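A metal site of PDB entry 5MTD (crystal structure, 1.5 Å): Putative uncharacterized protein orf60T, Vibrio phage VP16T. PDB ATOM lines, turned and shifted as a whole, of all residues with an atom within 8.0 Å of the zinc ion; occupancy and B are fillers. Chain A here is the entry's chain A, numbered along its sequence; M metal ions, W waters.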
ATOM      1  N   LEU A  11     -12.230   2.435  15.993  1.00  0.00           N
ATOM      2  CA  LEU A  11     -12.362   2.999  14.652  1.00  0.00           C
ATOM      3  C   LEU A  11     -12.161   1.968  13.540  1.00  0.00           C
ATOM      4  O   LEU A  11     -12.604   2.183  12.404  1.00  0.00           O
ATOM      5  CB  LEU A  11     -11.415   4.202  14.444  1.00  0.00           C
ATOM      6  CG  LEU A  11     -11.773   5.415  15.319  1.00  0.00           C
ATOM      7  CD1 LEU A  11     -10.754   6.532  15.169  1.00  0.00           C
ATOM      8  CD2 LEU A  11     -13.186   5.935  15.013  1.00  0.00           C
ATOM      9  N   GLY A  42     -22.137  14.301  10.326  1.00  0.00           N
ATOM     10  CA  GLY A  42     -22.446  12.875  10.429  1.00  0.00           C
ATOM     11  C   GLY A  42     -21.613  12.281  11.540  1.00  0.00           C
ATOM     12  O   GLY A  42     -20.575  12.832  11.913  1.00  0.00           O
ATOM     13  N   LEU A  43     -22.074  11.158  12.081  1.00  0.00           N
ATOM     14  CA  LEU A  43     -21.352  10.443  13.125  1.00  0.00           C
ATOM     15  C   LEU A  43     -21.794   8.989  13.165  1.00  0.00           C
ATOM     16  O   LEU A  43     -22.974   8.705  12.979  1.00  0.00           O
ATOM     17  CB  LEU A  43     -21.569  11.118  14.488  1.00  0.00           C
ATOM     18  CG  LEU A  43     -20.701  10.551  15.615  1.00  0.00           C
ATOM     19  CD1 LEU A  43     -19.282  11.129  15.544  1.00  0.00           C
ATOM     20  CD2 LEU A  43     -21.342  10.844  16.981  1.00  0.00           C
ATOM     21  N   ALA A  44     -20.852   8.070  13.397  1.00  0.00           N
ATOM     22  CA  ALA A  44     -21.162   6.653  13.476  1.00  0.00           C
ATOM     23  C   ALA A  44     -20.834   6.132  14.865  1.00  0.00           C
ATOM     24  O   ALA A  44     -19.958   6.693  15.533  1.00  0.00           O
ATOM     25  CB  ALA A  44     -20.357   5.898  12.448  1.00  0.00           C
ATOM     26  N   GLN A  47     -17.283   5.861  16.406  1.00  0.00           N
ATOM     27  CA  GLN A  47     -16.512   7.079  16.685  1.00  0.00           C
ATOM     28  C   GLN A  47     -16.661   7.567  18.118  1.00  0.00           C
ATOM     29  O   GLN A  47     -15.860   8.383  18.595  1.00  0.00           O
ATOM     30  CB  GLN A  47     -16.944   8.200  15.742  1.00  0.00           C
ATOM     31  CG  GLN A  47     -16.658   7.939  14.285  1.00  0.00           C
ATOM     32  CD  GLN A  47     -17.049   9.149  13.495  1.00  0.00           C
ATOM     33  OE1 GLN A  47     -18.201   9.251  13.052  1.00  0.00           O
ATOM     34  NE2 GLN A  47     -16.138  10.085  13.332  1.00  0.00           N
ATOM     35  N   GLU A  83     -13.372  14.877   1.827  1.00  0.00           N
ATOM     36  CA  GLU A  83     -14.023  14.648   3.109  1.00  0.00           C
ATOM     37  C   GLU A  83     -13.093  14.849   4.264  1.00  0.00           C
ATOM     38  O   GLU A  83     -11.926  14.477   4.211  1.00  0.00           O
ATOM     39  CB  GLU A  83     -14.548  13.211   3.164  1.00  0.00           C
ATOM     40  CG  GLU A  83     -15.526  12.904   2.044  1.00  0.00           C
ATOM     41  CD  GLU A  83     -16.037  11.476   2.044  1.00  0.00           C
ATOM     42  OE1 GLU A  83     -15.820  10.717   3.013  1.00  0.00           O
ATOM     43  OE2 GLU A  83     -16.705  11.101   1.064  1.00  0.00           O
ATOM     44  N   GLY A  84     -13.632  15.439   5.338  1.00  0.00           N
ATOM     45  CA  GLY A  84     -12.998  15.359   6.634  1.00  0.00           C
ATOM     46  C   GLY A  84     -13.685  14.292   7.473  1.00  0.00           C
ATOM     47  O   GLY A  84     -14.488  13.506   6.986  1.00  0.00           O
ATOM     48  N   CYS A  85     -13.318  14.267   8.743  1.00  0.00           N
ATOM     49  CA  CYS A  85     -13.844  13.297   9.677  1.00  0.00           C
ATOM     50  C   CYS A  85     -13.611  13.799  11.081  1.00  0.00           C
ATOM     51  O   CYS A  85     -12.511  14.283  11.393  1.00  0.00           O
ATOM     52  CB  CYS A  85     -13.157  11.944   9.496  1.00  0.00           C
ATOM     53  SG  CYS A  85     -13.781  10.643  10.579  1.00  0.00           S
ATOM     54  N   LEU A  86     -14.626  13.667  11.931  1.00  0.00           N
ATOM     55  CA  LEU A  86     -14.504  14.150  13.308  1.00  0.00           C
ATOM     56  C   LEU A  86     -13.437  13.388  14.077  1.00  0.00           C
ATOM     57  O   LEU A  86     -12.872  13.932  15.031  1.00  0.00           O
ATOM     58  CB  LEU A  86     -15.849  14.057  14.029  1.00  0.00           C
ATOM     59  CG  LEU A  86     -16.959  14.987  13.513  1.00  0.00           C
ATOM     60  CD1 LEU A  86     -18.218  14.737  14.328  1.00  0.00           C
ATOM     61  CD2 LEU A  86     -16.553  16.447  13.587  1.00  0.00           C
ATOM     62  N   SER A  87     -13.147  12.158  13.659  1.00  0.00           N
ATOM     63  CA  SER A  87     -12.120  11.348  14.310  1.00  0.00           C
ATOM     64  C   SER A  87     -10.713  11.741  13.878  1.00  0.00           C
ATOM     65  O   SER A  87      -9.739  11.389  14.555  1.00  0.00           O
ATOM     66  CB  SER A  87     -12.346   9.878  13.989  1.00  0.00           C
ATOM     67  OG  SER A  87     -13.593   9.441  14.464  1.00  0.00           O
ATOM     68  N   TYR A  88     -10.599  12.507  12.796  1.00  0.00           N
ATOM     69  CA  TYR A  88      -9.283  12.917  12.267  1.00  0.00           C
ATOM     70  C   TYR A  88      -9.260  14.418  12.023  1.00  0.00           C
ATOM     71  O   TYR A  88      -9.162  14.873  10.891  1.00  0.00           O
ATOM     72  CB  TYR A  88      -8.934  12.141  10.985  1.00  0.00           C
ATOM     73  CG  TYR A  88      -9.003  10.654  11.187  1.00  0.00           C
ATOM     74  CD1 TYR A  88     -10.122   9.930  10.807  1.00  0.00           C
ATOM     75  CD2 TYR A  88      -7.953   9.962  11.817  1.00  0.00           C
ATOM     76  CE1 TYR A  88     -10.202   8.564  11.009  1.00  0.00           C
ATOM     77  CE2 TYR A  88      -8.024   8.586  12.036  1.00  0.00           C
ATOM     78  CZ  TYR A  88      -9.151   7.892  11.616  1.00  0.00           C
ATOM     79  OH  TYR A  88      -9.262   6.529  11.825  1.00  0.00           O
ATOM     80  N   ARG A  97     -16.437   8.178  -4.359  1.00  0.00           N
ATOM     81  CA  ARG A  97     -17.743   7.808  -3.800  1.00  0.00           C
ATOM     82  C   ARG A  97     -18.708   7.550  -4.926  1.00  0.00           C
ATOM     83  O   ARG A  97     -18.515   8.037  -6.042  1.00  0.00           O
ATOM     84  CB  ARG A  97     -18.284   8.958  -2.946  1.00  0.00           C
ATOM     85  CG  ARG A  97     -17.496   9.235  -1.669  1.00  0.00           C
ATOM     86  CD  ARG A  97     -17.610   8.075  -0.696  1.00  0.00           C
ATOM     87  NE  ARG A  97     -16.992   8.409   0.580  1.00  0.00           N
ATOM     88  CZ  ARG A  97     -16.619   7.524   1.498  1.00  0.00           C
ATOM     89  NH1 ARG A  97     -16.772   6.219   1.292  1.00  0.00           N
ATOM     90  NH2 ARG A  97     -16.076   7.933   2.635  1.00  0.00           N
ATOM     91  N   CYS A 124     -21.896  11.617   2.675  1.00  0.00           N
ATOM     92  CA  CYS A 124     -22.176  11.565   4.139  1.00  0.00           C
ATOM     93  C   CYS A 124     -22.524  10.107   4.495  1.00  0.00           C
ATOM     94  O   CYS A 124     -21.882   9.437   5.356  1.00  0.00           O
ATOM     95  CB  CYS A 124     -23.430  12.451   4.369  1.00  0.00           C
ATOM     96  SG  CYS A 124     -23.208  14.241   4.588  1.00  0.00           S
ATOM     97  N   HIS A 127     -19.716   7.523   3.931  1.00  0.00           N
ATOM     98  CA  HIS A 127     -18.677   7.762   4.930  1.00  0.00           C
ATOM     99  C   HIS A 127     -19.094   7.159   6.279  1.00  0.00           C
ATOM    100  O   HIS A 127     -18.299   6.492   6.946  1.00  0.00           O
ATOM    101  CB  HIS A 127     -18.439   9.258   5.070  1.00  0.00           C
ATOM    102  CG  HIS A 127     -17.420   9.640   6.088  1.00  0.00           C
ATOM    103  ND1 HIS A 127     -16.253  10.288   5.738  1.00  0.00           N
ATOM    104  CD2 HIS A 127     -17.398   9.529   7.441  1.00  0.00           C
ATOM    105  CE1 HIS A 127     -15.563  10.572   6.829  1.00  0.00           C
ATOM    106  NE2 HIS A 127     -16.226  10.108   7.877  1.00  0.00           N
ATOM    107  N   GLU A 128     -20.329   7.403   6.693  1.00  0.00           N
ATOM    108  CA  GLU A 128     -20.758   6.881   8.007  1.00  0.00           C
ATOM    109  C   GLU A 128     -20.922   5.380   8.032  1.00  0.00           C
ATOM    110  O   GLU A 128     -20.599   4.732   9.023  1.00  0.00           O
ATOM    111  CB  GLU A 128     -22.019   7.581   8.535  1.00  0.00           C
ATOM    112  CG  GLU A 128     -21.913   9.109   8.603  1.00  0.00           C
ATOM    113  CD  GLU A 128     -20.704   9.610   9.350  1.00  0.00           C
ATOM    114  OE1 GLU A 128     -20.245  10.737   9.043  1.00  0.00           O
ATOM    115  OE2 GLU A 128     -20.218   8.885  10.255  1.00  0.00           O
ATOM    116  N   ASP A 130     -19.231   3.353   6.162  1.00  0.00           N
ATOM    117  CA  ASP A 130     -17.839   2.861   6.191  1.00  0.00           C
ATOM    118  C   ASP A 130     -17.353   2.727   7.642  1.00  0.00           C
ATOM    119  O   ASP A 130     -16.744   1.721   7.997  1.00  0.00           O
ATOM    120  CB  ASP A 130     -16.895   3.815   5.452  1.00  0.00           C
ATOM    121  CG  ASP A 130     -16.842   3.555   3.957  1.00  0.00           C
ATOM    122  OD1 ASP A 130     -17.516   2.616   3.458  1.00  0.00           O
ATOM    123  OD2 ASP A 130     -16.104   4.319   3.296  1.00  0.00           O
ATOM    124  N   HIS A 131     -17.606   3.748   8.472  1.00  0.00           N
ATOM    125  CA  HIS A 131     -17.184   3.680   9.881  1.00  0.00           C
ATOM    126  C   HIS A 131     -17.642   2.388  10.553  1.00  0.00           C
ATOM    127  O   HIS A 131     -16.910   1.819  11.353  1.00  0.00           O
ATOM    128  CB  HIS A 131     -17.730   4.869  10.681  1.00  0.00           C
ATOM    129  CG  HIS A 131     -16.864   6.103  10.626  1.00  0.00           C
ATOM    130  ND1 HIS A 131     -15.555   6.127  11.074  1.00  0.00           N
ATOM    131  CD2 HIS A 131     -17.148   7.359  10.205  1.00  0.00           C
ATOM    132  CE1 HIS A 131     -15.063   7.354  10.902  1.00  0.00           C
ATOM    133  NE2 HIS A 131     -16.012   8.118  10.390  1.00  0.00           N
ATOM    134  N   VAL A 135     -13.895   1.178   8.501  1.00  0.00           N
ATOM    135  CA  VAL A 135     -13.217   1.810   7.371  1.00  0.00           C
ATOM    136  C   VAL A 135     -13.253   3.323   7.557  1.00  0.00           C
ATOM    137  O   VAL A 135     -14.322   3.900   7.781  1.00  0.00           O
ATOM    138  CB  VAL A 135     -13.900   1.402   6.038  1.00  0.00           C
ATOM    139  CG1 VAL A 135     -13.304   2.160   4.845  1.00  0.00           C
ATOM    140  CG2 VAL A 135     -13.775  -0.100   5.823  1.00  0.00           C
ATOM    141  N   THR A 136     -12.069   3.943   7.476  1.00  0.00           N
ATOM    142  CA  THR A 136     -11.904   5.368   7.702  1.00  0.00           C
ATOM    143  C   THR A 136     -11.208   6.037   6.516  1.00  0.00           C
ATOM    144  O   THR A 136     -10.599   5.354   5.676  1.00  0.00           O
ATOM    145  CB  THR A 136     -11.085   5.642   8.973  1.00  0.00           C
ATOM    146  OG1 THR A 136      -9.782   5.055   8.831  1.00  0.00           O
ATOM    147  CG2 THR A 136     -11.761   5.022  10.184  1.00  0.00           C
ATOM    148  N   ILE A 137     -11.319   7.352   6.414  1.00  0.00           N
ATOM    149  CA  ILE A 137     -10.717   8.091   5.275  1.00  0.00           C
ATOM    150  C   ILE A 137      -9.177   8.097   5.330  1.00  0.00           C
ATOM    151  O   ILE A 137      -8.604   8.050   6.419  1.00  0.00           O
ATOM    152  CB  ILE A 137     -11.262   9.527   5.189  1.00  0.00           C
ATOM    153  CG1 ILE A 137     -10.970  10.294   6.488  1.00  0.00           C
ATOM    154  CG2 ILE A 137     -12.772   9.514   4.872  1.00  0.00           C
ATOM    155  CD1 ILE A 137     -11.185  11.809   6.374  1.00  0.00           C
ATOM    156  OXT ILE A 137      -8.600   8.207   4.238  1.00  0.00           O
HETATM  157 ZN    ZN M   1     -15.843  10.083   9.880  1.00  0.00          ZN
HETATM  158  O   HOH W   1     -17.846  10.652  10.400  1.00  0.00           O
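A ring nitrogen (NE2) of His 131 binds the zinc ion, at 2.0 Å. A ring nitrogen (NE2) of His 127 binds the zinc ion (2.0 Å). Water W1 is bound to the zinc ion. The zinc ion is bound by the side-chain sulfur (SG) of Cys 85 (2.2 Å). The zinc ion has four donor atoms within binding distance.
The side-chain carboxylate (OE1) of Glu 83 sits at hydrogen-bond distance from a ring nitrogen (ND1) of His 127. The side-chain amide nitrogen of Gln 47 lies close to the side-chain sulfur of Cys 85. The side-chain sulfur of Cys 85 sits close to the backbone NH of Ser 87 (3.5 Å). OE1 of Gln 47 lies close to OE2 of Glu 128, at 3.5 Å. NE2 of Gln 47 lies within hydrogen-bond range of OG of Ser 87. The side-chain amide oxygen (OE1) of Gln 47 lies within hydrogen-bond range of the backbone NH (N) of Ala 44 (2.9 Å).
Water W1 bridges the side-chain carboxylate (OE1) of Glu 128 (2.8 Å) and the side-chain amide oxygen (OE1) of Gln 47 (3.0 Å).
Merely in contact with the zinc ion: Gln 47 (3.5 Å). Within 4 Å of the zinc ion: Gln 47, Cys 85, His 127 and His 131. The nearest printed residue that does not touch the zinc ion is Leu 86 (4.3 Å).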
